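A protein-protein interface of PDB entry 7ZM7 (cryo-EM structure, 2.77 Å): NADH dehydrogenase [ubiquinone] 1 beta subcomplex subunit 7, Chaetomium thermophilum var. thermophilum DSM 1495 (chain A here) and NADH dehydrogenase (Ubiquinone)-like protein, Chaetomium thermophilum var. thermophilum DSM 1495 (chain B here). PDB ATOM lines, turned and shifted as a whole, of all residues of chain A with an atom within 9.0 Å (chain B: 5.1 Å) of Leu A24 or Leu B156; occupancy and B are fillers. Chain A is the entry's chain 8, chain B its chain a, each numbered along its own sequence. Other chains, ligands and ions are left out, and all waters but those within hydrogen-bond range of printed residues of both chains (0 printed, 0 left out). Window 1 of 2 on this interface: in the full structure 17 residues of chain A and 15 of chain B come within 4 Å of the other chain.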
ATOM      1  N   ALA A  12     -21.985  16.309  18.753  1.00  0.00           N
ATOM      2  CA  ALA A  12     -21.637  14.897  18.681  1.00  0.00           C
ATOM      3  C   ALA A  12     -22.791  14.049  19.199  1.00  0.00           C
ATOM      4  O   ALA A  12     -23.244  14.228  20.333  1.00  0.00           O
ATOM      5  CB  ALA A  12     -20.369  14.622  19.484  1.00  0.00           C
ATOM      6  N   THR A  13     -23.224  13.087  18.374  1.00  0.00           N
ATOM      7  CA  THR A  13     -24.412  12.255  18.708  1.00  0.00           C
ATOM      8  C   THR A  13     -24.177  11.340  19.912  1.00  0.00           C
ATOM      9  O   THR A  13     -23.009  11.056  20.223  1.00  0.00           O
ATOM     10  CB  THR A  13     -24.827  11.395  17.510  1.00  0.00           C
ATOM     11  OG1 THR A  13     -23.989  10.239  17.483  1.00  0.00           O
ATOM     12  CG2 THR A  13     -24.734  12.136  16.194  1.00  0.00           C
ATOM     13  N   ARG A  14     -25.265  10.866  20.524  1.00  0.00           N
ATOM     14  CA  ARG A  14     -25.181   9.991  21.723  1.00  0.00           C
ATOM     15  C   ARG A  14     -24.473   8.681  21.367  1.00  0.00           C
ATOM     16  O   ARG A  14     -23.680   8.196  22.194  1.00  0.00           O
ATOM     17  CB  ARG A  14     -26.611   9.712  22.192  1.00  0.00           C
ATOM     18  CG  ARG A  14     -26.759   9.425  23.678  1.00  0.00           C
ATOM     19  CD  ARG A  14     -28.231   9.365  24.048  1.00  0.00           C
ATOM     20  NE  ARG A  14     -29.048   8.838  22.965  1.00  0.00           N
ATOM     21  CZ  ARG A  14     -29.422   7.568  22.845  1.00  0.00           C
ATOM     22  NH1 ARG A  14     -30.164   7.191  21.819  1.00  0.00           N
ATOM     23  NH2 ARG A  14     -29.058   6.682  23.752  1.00  0.00           N
ATOM     24  N   GLU A  15     -24.776   8.118  20.194  1.00  0.00           N
ATOM     25  CA  GLU A  15     -24.147   6.842  19.767  1.00  0.00           C
ATOM     26  C   GLU A  15     -22.643   7.055  19.592  1.00  0.00           C
ATOM     27  O   GLU A  15     -21.868   6.205  20.064  1.00  0.00           O
ATOM     28  CB  GLU A  15     -24.747   6.389  18.435  1.00  0.00           C
ATOM     29  CG  GLU A  15     -26.248   6.583  18.353  1.00  0.00           C
ATOM     30  CD  GLU A  15     -27.064   5.587  19.160  1.00  0.00           C
ATOM     31  OE1 GLU A  15     -26.576   4.459  19.370  1.00  0.00           O
ATOM     32  OE2 GLU A  15     -28.182   5.946  19.581  1.00  0.00           O
ATOM     33  N   MET A  17     -20.821   9.320  20.989  1.00  0.00           N
ATOM     34  CA  MET A  17     -20.217   9.631  22.308  1.00  0.00           C
ATOM     35  C   MET A  17     -19.885   8.355  23.074  1.00  0.00           C
ATOM     36  O   MET A  17     -18.866   8.364  23.789  1.00  0.00           O
ATOM     37  CB  MET A  17     -21.161  10.480  23.158  1.00  0.00           C
ATOM     38  CG  MET A  17     -21.069  11.948  22.835  1.00  0.00           C
ATOM     39  SD  MET A  17     -22.074  12.948  23.941  1.00  0.00           S
ATOM     40  CE  MET A  17     -21.711  14.578  23.295  1.00  0.00           C
ATOM     41  N   ARG A  18     -20.692   7.296  22.935  1.00  0.00           N
ATOM     42  CA  ARG A  18     -20.377   6.144  23.767  1.00  0.00           C
ATOM     43  C   ARG A  18     -19.191   5.362  23.231  1.00  0.00           C
ATOM     44  O   ARG A  18     -18.520   4.665  23.996  1.00  0.00           O
ATOM     45  CB  ARG A  18     -21.595   5.228  23.879  1.00  0.00           C
ATOM     46  CG  ARG A  18     -21.698   4.206  22.767  1.00  0.00           C
ATOM     47  CD  ARG A  18     -22.586   3.059  23.142  1.00  0.00           C
ATOM     48  NE  ARG A  18     -22.848   2.188  22.001  1.00  0.00           N
ATOM     49  CZ  ARG A  18     -23.967   2.202  21.283  1.00  0.00           C
ATOM     50  NH1 ARG A  18     -24.109   1.371  20.260  1.00  0.00           N
ATOM     51  NH2 ARG A  18     -24.944   3.044  21.587  1.00  0.00           N
ATOM     52  N   LYS A  21     -16.035   6.346  24.854  1.00  0.00           N
ATOM     53  CA  LYS A  21     -16.033   6.132  26.298  1.00  0.00           C
ATOM     54  C   LYS A  21     -15.809   7.435  27.057  1.00  0.00           C
ATOM     55  O   LYS A  21     -15.069   7.484  28.041  1.00  0.00           O
ATOM     56  CB  LYS A  21     -14.986   5.093  26.693  1.00  0.00           C
ATOM     57  CG  LYS A  21     -15.304   3.694  26.224  1.00  0.00           C
ATOM     58  CD  LYS A  21     -14.197   2.740  26.594  1.00  0.00           C
ATOM     59  CE  LYS A  21     -14.196   2.523  28.093  1.00  0.00           C
ATOM     60  NZ  LYS A  21     -15.418   1.785  28.499  1.00  0.00           N
ATOM     61  N   VAL A  22     -16.440   8.499  26.586  1.00  0.00           N
ATOM     62  CA  VAL A  22     -16.448   9.764  27.326  1.00  0.00           C
ATOM     63  C   VAL A  22     -17.200   9.570  28.638  1.00  0.00           C
ATOM     64  O   VAL A  22     -18.170   8.798  28.680  1.00  0.00           O
ATOM     65  CB  VAL A  22     -17.070  10.865  26.462  1.00  0.00           C
ATOM     66  CG1 VAL A  22     -18.511  10.577  26.178  1.00  0.00           C
ATOM     67  CG2 VAL A  22     -16.938  12.220  27.118  1.00  0.00           C
ATOM     68  N   PRO A  23     -16.752  10.170  29.740  1.00  0.00           N
ATOM     69  CA  PRO A  23     -17.401   9.919  31.028  1.00  0.00           C
ATOM     70  C   PRO A  23     -18.834  10.416  31.042  1.00  0.00           C
ATOM     71  O   PRO A  23     -19.186  11.391  30.378  1.00  0.00           O
ATOM     72  CB  PRO A  23     -16.529  10.692  32.016  1.00  0.00           C
ATOM     73  CG  PRO A  23     -15.214  10.771  31.359  1.00  0.00           C
ATOM     74  CD  PRO A  23     -15.490  10.906  29.910  1.00  0.00           C
ATOM     75  N   LEU A  24     -19.660   9.737  31.834  1.00  0.00           N
ATOM     76  CA  LEU A  24     -21.104   9.812  31.642  1.00  0.00           C
ATOM     77  C   LEU A  24     -21.638  11.220  31.843  1.00  0.00           C
ATOM     78  O   LEU A  24     -22.372  11.736  30.998  1.00  0.00           O
ATOM     79  CB  LEU A  24     -21.808   8.834  32.573  1.00  0.00           C
ATOM     80  CG  LEU A  24     -21.912   7.457  31.944  1.00  0.00           C
ATOM     81  CD1 LEU A  24     -22.652   6.487  32.843  1.00  0.00           C
ATOM     82  CD2 LEU A  24     -22.601   7.586  30.629  1.00  0.00           C
ATOM     83  N   ALA A  25     -21.279  11.861  32.953  1.00  0.00           N
ATOM     84  CA  ALA A  25     -21.855  13.165  33.262  1.00  0.00           C
ATOM     85  C   ALA A  25     -21.384  14.242  32.302  1.00  0.00           C
ATOM     86  O   ALA A  25     -21.927  15.347  32.318  1.00  0.00           O
ATOM     87  CB  ALA A  25     -21.526  13.561  34.697  1.00  0.00           C
ATOM     88  N   TYR A  26     -20.388  13.948  31.472  1.00  0.00           N
ATOM     89  CA  TYR A  26     -19.857  14.902  30.513  1.00  0.00           C
ATOM     90  C   TYR A  26     -20.319  14.617  29.101  1.00  0.00           C
ATOM     91  O   TYR A  26     -19.689  15.076  28.153  1.00  0.00           O
ATOM     92  CB  TYR A  26     -18.335  14.904  30.569  1.00  0.00           C
ATOM     93  CG  TYR A  26     -17.798  15.378  31.887  1.00  0.00           C
ATOM     94  CD1 TYR A  26     -18.494  16.303  32.647  1.00  0.00           C
ATOM     95  CD2 TYR A  26     -16.606  14.884  32.388  1.00  0.00           C
ATOM     96  CE1 TYR A  26     -18.013  16.734  33.857  1.00  0.00           C
ATOM     97  CE2 TYR A  26     -16.115  15.309  33.600  1.00  0.00           C
ATOM     98  CZ  TYR A  26     -16.821  16.234  34.329  1.00  0.00           C
ATOM     99  OH  TYR A  26     -16.333  16.658  35.540  1.00  0.00           O
ATOM    100  N   ARG A  27     -21.398  13.868  28.932  1.00  0.00           N
ATOM    101  CA  ARG A  27     -21.933  13.616  27.598  1.00  0.00           C
ATOM    102  C   ARG A  27     -22.929  14.688  27.212  1.00  0.00           C
ATOM    103  O   ARG A  27     -23.978  14.433  26.637  1.00  0.00           O
ATOM    104  CB  ARG A  27     -22.558  12.234  27.544  1.00  0.00           C
ATOM    105  CG  ARG A  27     -21.529  11.152  27.644  1.00  0.00           C
ATOM    106  CD  ARG A  27     -22.113   9.797  27.547  1.00  0.00           C
ATOM    107  NE  ARG A  27     -21.142   8.807  27.971  1.00  0.00           N
ATOM    108  CZ  ARG A  27     -21.059   7.588  27.463  1.00  0.00           C
ATOM    109  NH1 ARG A  27     -21.896   7.206  26.512  1.00  0.00           N
ATOM    110  NH2 ARG A  27     -20.142   6.751  27.908  1.00  0.00           N
ATOM    111  N   ASP A  28     -22.551  15.922  27.501  1.00  0.00           N
ATOM    112  CA  ASP A  28     -23.420  17.071  27.351  1.00  0.00           C
ATOM    113  C   ASP A  28     -23.282  17.645  25.946  1.00  0.00           C
ATOM    114  O   ASP A  28     -22.661  17.050  25.062  1.00  0.00           O
ATOM    115  CB  ASP A  28     -23.107  18.092  28.444  1.00  0.00           C
ATOM    116  CG  ASP A  28     -21.688  18.629  28.354  1.00  0.00           C
ATOM    117  OD1 ASP A  28     -20.930  18.180  27.468  1.00  0.00           O
ATOM    118  OD2 ASP A  28     -21.326  19.505  29.169  1.00  0.00           O
ATOM    119  N   SER A  29     -23.859  18.828  25.740  1.00  0.00           N
ATOM    120  CA  SER A  29     -23.956  19.403  24.406  1.00  0.00           C
ATOM    121  C   SER A  29     -22.598  19.797  23.847  1.00  0.00           C
ATOM    122  O   SER A  29     -22.416  19.814  22.625  1.00  0.00           O
ATOM    123  CB  SER A  29     -24.874  20.620  24.448  1.00  0.00           C
ATOM    124  OG  SER A  29     -24.334  21.612  25.304  1.00  0.00           O
ATOM    125  N   ALA A  31     -19.441  18.345  24.410  1.00  0.00           N
ATOM    126  CA  ALA A  31     -18.410  17.339  24.627  1.00  0.00           C
ATOM    127  C   ALA A  31     -17.769  16.860  23.342  1.00  0.00           C
ATOM    128  O   ALA A  31     -16.909  15.980  23.392  1.00  0.00           O
ATOM    129  CB  ALA A  31     -18.983  16.137  25.372  1.00  0.00           C
ATOM    130  N   LEU A  34     -14.393  17.197  24.019  1.00  0.00           N
ATOM    131  CA  LEU A  34     -13.785  16.302  24.997  1.00  0.00           C
ATOM    132  C   LEU A  34     -13.166  15.095  24.324  1.00  0.00           C
ATOM    133  O   LEU A  34     -12.166  14.555  24.808  1.00  0.00           O
ATOM    134  CB  LEU A  34     -14.808  15.841  26.022  1.00  0.00           C
ATOM    135  CG  LEU A  34     -14.195  15.258  27.286  1.00  0.00           C
ATOM    136  CD1 LEU A  34     -13.090  16.127  27.801  1.00  0.00           C
ATOM    137  CD2 LEU A  34     -15.264  15.099  28.325  1.00  0.00           C
ATOM    138  N   ASN A  38      -9.471  14.358  25.461  1.00  0.00           N
ATOM    139  CA  ASN A  38      -9.064  13.104  26.078  1.00  0.00           C
ATOM    140  C   ASN A  38      -8.098  12.348  25.177  1.00  0.00           C
ATOM    141  O   ASN A  38      -7.135  11.745  25.654  1.00  0.00           O
ATOM    142  CB  ASN A  38     -10.298  12.266  26.388  1.00  0.00           C
ATOM    143  CG  ASN A  38     -10.990  12.699  27.662  1.00  0.00           C
ATOM    144  OD1 ASN A  38     -10.519  13.587  28.368  1.00  0.00           O
ATOM    145  ND2 ASN A  38     -12.130  12.086  27.952  1.00  0.00           N
ATOM    146  N   PHE B 152     -29.572  17.401  29.635  1.00  0.00           N
ATOM    147  CA  PHE B 152     -29.073  16.322  28.806  1.00  0.00           C
ATOM    148  C   PHE B 152     -30.142  15.937  27.801  1.00  0.00           C
ATOM    149  O   PHE B 152     -31.334  15.912  28.116  1.00  0.00           O
ATOM    150  CB  PHE B 152     -28.688  15.106  29.635  1.00  0.00           C
ATOM    151  CG  PHE B 152     -27.382  15.248  30.333  1.00  0.00           C
ATOM    152  CD1 PHE B 152     -26.212  14.882  29.696  1.00  0.00           C
ATOM    153  CD2 PHE B 152     -27.318  15.743  31.622  1.00  0.00           C
ATOM    154  CE1 PHE B 152     -25.002  15.004  30.325  1.00  0.00           C
ATOM    155  CE2 PHE B 152     -26.110  15.869  32.260  1.00  0.00           C
ATOM    156  CZ  PHE B 152     -24.946  15.497  31.606  1.00  0.00           C
ATOM    157  N   GLU B 153     -29.707  15.638  26.584  1.00  0.00           N
ATOM    158  CA  GLU B 153     -30.632  15.297  25.512  1.00  0.00           C
ATOM    159  C   GLU B 153     -31.103  13.859  25.699  1.00  0.00           C
ATOM    160  O   GLU B 153     -30.301  12.919  25.698  1.00  0.00           O
ATOM    161  CB  GLU B 153     -29.985  15.556  24.152  1.00  0.00           C
ATOM    162  CG  GLU B 153     -28.730  14.768  23.846  1.00  0.00           C
ATOM    163  CD  GLU B 153     -29.018  13.411  23.262  1.00  0.00           C
ATOM    164  OE1 GLU B 153     -30.136  13.207  22.749  1.00  0.00           O
ATOM    165  OE2 GLU B 153     -28.131  12.541  23.334  1.00  0.00           O
ATOM    166  N   GLY B 154     -32.403  13.699  25.931  1.00  0.00           N
ATOM    167  CA  GLY B 154     -33.004  12.409  26.181  1.00  0.00           C
ATOM    168  C   GLY B 154     -32.856  11.903  27.594  1.00  0.00           C
ATOM    169  O   GLY B 154     -33.358  10.815  27.902  1.00  0.00           O
ATOM    170  N   GLY B 155     -32.184  12.647  28.464  1.00  0.00           N
ATOM    171  CA  GLY B 155     -31.989  12.210  29.824  1.00  0.00           C
ATOM    172  C   GLY B 155     -30.942  11.139  29.997  1.00  0.00           C
ATOM    173  O   GLY B 155     -30.725  10.689  31.126  1.00  0.00           O
ATOM    174  N   LEU B 156     -30.285  10.723  28.916  1.00  0.00           N
ATOM    175  CA  LEU B 156     -29.325   9.622  28.947  1.00  0.00           C
ATOM    176  C   LEU B 156     -29.951   8.370  29.549  1.00  0.00           C
ATOM    177  O   LEU B 156     -29.283   7.568  30.203  1.00  0.00           O
ATOM    178  CB  LEU B 156     -28.054  10.011  29.699  1.00  0.00           C
ATOM    179  CG  LEU B 156     -27.216  11.106  29.052  1.00  0.00           C
ATOM    180  CD1 LEU B 156     -26.057  11.477  29.951  1.00  0.00           C
ATOM    181  CD2 LEU B 156     -26.724  10.654  27.692  1.00  0.00           C
ATOM    182  N   GLU B 157     -31.252   8.198  29.317  1.00  0.00           N
ATOM    183  CA  GLU B 157     -31.952   7.053  29.879  1.00  0.00           C
ATOM    184  C   GLU B 157     -31.394   5.732  29.375  1.00  0.00           C
ATOM    185  O   GLU B 157     -31.482   4.725  30.085  1.00  0.00           O
ATOM    186  CB  GLU B 157     -33.449   7.166  29.581  1.00  0.00           C
ATOM    187  CG  GLU B 157     -33.797   7.324  28.108  1.00  0.00           C
ATOM    188  CD  GLU B 157     -33.985   6.005  27.395  1.00  0.00           C
ATOM    189  OE1 GLU B 157     -34.204   4.986  28.080  1.00  0.00           O
ATOM    190  OE2 GLU B 157     -33.928   5.988  26.148  1.00  0.00           O
ATOM    191  N   ARG B 158     -30.763   5.697  28.235  1.00  0.00           N
ATOM    192  CA  ARG B 158     -30.209   4.431  27.685  1.00  0.00           C
ATOM    193  C   ARG B 158     -28.797   4.215  28.236  1.00  0.00           C
ATOM    194  O   ARG B 158     -28.309   3.077  28.152  1.00  0.00           O
ATOM    195  CB  ARG B 158     -30.225   4.480  26.153  1.00  0.00           C
ATOM    196  CG  ARG B 158     -30.496   3.140  25.484  1.00  0.00           C
ATOM    197  CD  ARG B 158     -29.234   2.464  24.980  1.00  0.00           C
ATOM    198  NE  ARG B 158     -28.525   3.287  24.010  1.00  0.00           N
ATOM    199  CZ  ARG B 158     -28.708   3.228  22.695  1.00  0.00           C
ATOM    200  NH1 ARG B 158     -28.015   4.019  21.895  1.00  0.00           N
ATOM    201  NH2 ARG B 158     -29.580   2.378  22.186  1.00  0.00           N
ATOM    202  N   GLU B 159     -28.170   5.282  28.784  1.00  0.00           N
ATOM    203  CA  GLU B 159     -26.812   5.159  29.294  1.00  0.00           C
ATOM    204  C   GLU B 159     -26.746   5.024  30.806  1.00  0.00           C
ATOM    205  O   GLU B 159     -25.661   5.143  31.374  1.00  0.00           O
ATOM    206  CB  GLU B 159     -25.980   6.360  28.847  1.00  0.00           C
ATOM    207  CG  GLU B 159     -25.633   6.332  27.378  1.00  0.00           C
ATOM    208  CD  GLU B 159     -26.772   6.820  26.513  1.00  0.00           C
ATOM    209  OE1 GLU B 159     -27.787   7.277  27.076  1.00  0.00           O
ATOM    210  OE2 GLU B 159     -26.654   6.747  25.273  1.00  0.00           O
ATOM    211  N   LEU B 160     -27.868   4.791  31.473  1.00  0.00           N
ATOM    212  CA  LEU B 160     -27.886   4.701  32.924  1.00  0.00           C
ATOM    213  C   LEU B 160     -28.701   3.527  33.434  1.00  0.00           C
ATOM    214  O   LEU B 160     -28.892   3.406  34.647  1.00  0.00           O
ATOM    215  CB  LEU B 160     -28.409   6.002  33.533  1.00  0.00           C
ATOM    216  CG  LEU B 160     -27.435   7.169  33.397  1.00  0.00           C
ATOM    217  CD1 LEU B 160     -28.025   8.452  33.936  1.00  0.00           C
ATOM    218  CD2 LEU B 160     -26.155   6.819  34.109  1.00  0.00           C
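The guanidinium group (NE) of Arg A14 lies within salt-bridge range of the side-chain carboxylate (OE2) of Glu B153. NH2 of Arg A18 lies close to NH1 of Arg B158, 3.2 Å away. The guanidinium group of Arg B158 lies within salt-bridge range of the side-chain carboxylate of Glu A15 (2.9 Å). The guanidinium group (NH1) of Arg B158 sits close to the guanidinium group (NH2) of Arg A14 (3.4 Å). The side-chain carboxylate of Glu B159 is in salt-bridge range of the guanidinium group of Arg A14, 2.8 Å away.
The side-chain carboxylate of Asp A28 is in hydrogen-bond range of the backbone NH of Ala A31 (3.4 Å). OE1 of Glu A15 is in salt-bridge range of NH2 of Arg A18, at 3.1 Å. OE2 of Glu A15 is in salt-bridge range of NH1 of Arg A14. The backbone carbonyl oxygen (O) of Val A22 is in hydrogen-bond range of the guanidinium group (NH2) of Arg A27 (2.9 Å).
Leu B156 touches Leu A24 (CD1 to O, 3.8 Å). Glu B159 touches Leu A24. Leu B160 touches Leu A24 (CD2 to CD1, 3.7 Å). Phe B152 touches Ala A25 (CZ to O, 3.1 Å). Arg A27 touches Phe B152. Arg A27 touches Glu B159 (NH1 to CG, 3.9 Å). Phe B152 touches Asp A28.
Printed residues of chain B within 4 Å of Leu A24: Leu B156 (3.8 Å), Glu B159 (3.6 Å) and Leu B160 (3.7 Å). Leu B156 touches one residue of chain A. No residue of chain A comes within 4 Å of Gly B154. Of chain A, only Arg A14 (2.8 Å), Leu A24 (3.6 Å) and Arg A27 (3.9 Å) come within 4 Å of Glu B159. Printed residues of chain B within 4 Å of Arg A14: Glu B153, Arg B158 and Glu B159. Of the printed residues of chain A, Leu B160 touches Leu A24. Printed residues of chain A within 4 Å of Glu B153: Arg A14 (3.3 Å). Printed residues of chain A within 4 Å of Phe B152: Ala A25 (3.1 Å), Arg A27 (3.8 Å) and Asp A28 (3.9 Å). Glu B157 touches none of the printed residues of chain A. The nearest residue of chain A that does not touch Leu B156 is Arg A14 (4.1 Å). The nearest printed residue of chain B that does not touch Arg A27 is Leu B156 (4.3 Å).
Hydrophobic or aromatic side chains of chain B within 4 Å of the printed part of chain A: Phe B152, Leu B156 and Leu B160. Of the 18 printed residues of chain A, 7 touch a printed residue of chain B. Hydrophobic or aromatic side chains of chain A that line the printed part of chain B: Leu A24. Among the printed residues, 12 pairs touch across the chains. Among the printed residues, Asp or Glu carboxylates within 4 Å of a Lys or Arg side-chain nitrogen of the other chain: Arg A14 with Glu B153 (3.8 Å), Arg A14 with Glu B159 (2.8 Å) and Glu A15 with Arg B158 (2.9 Å).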
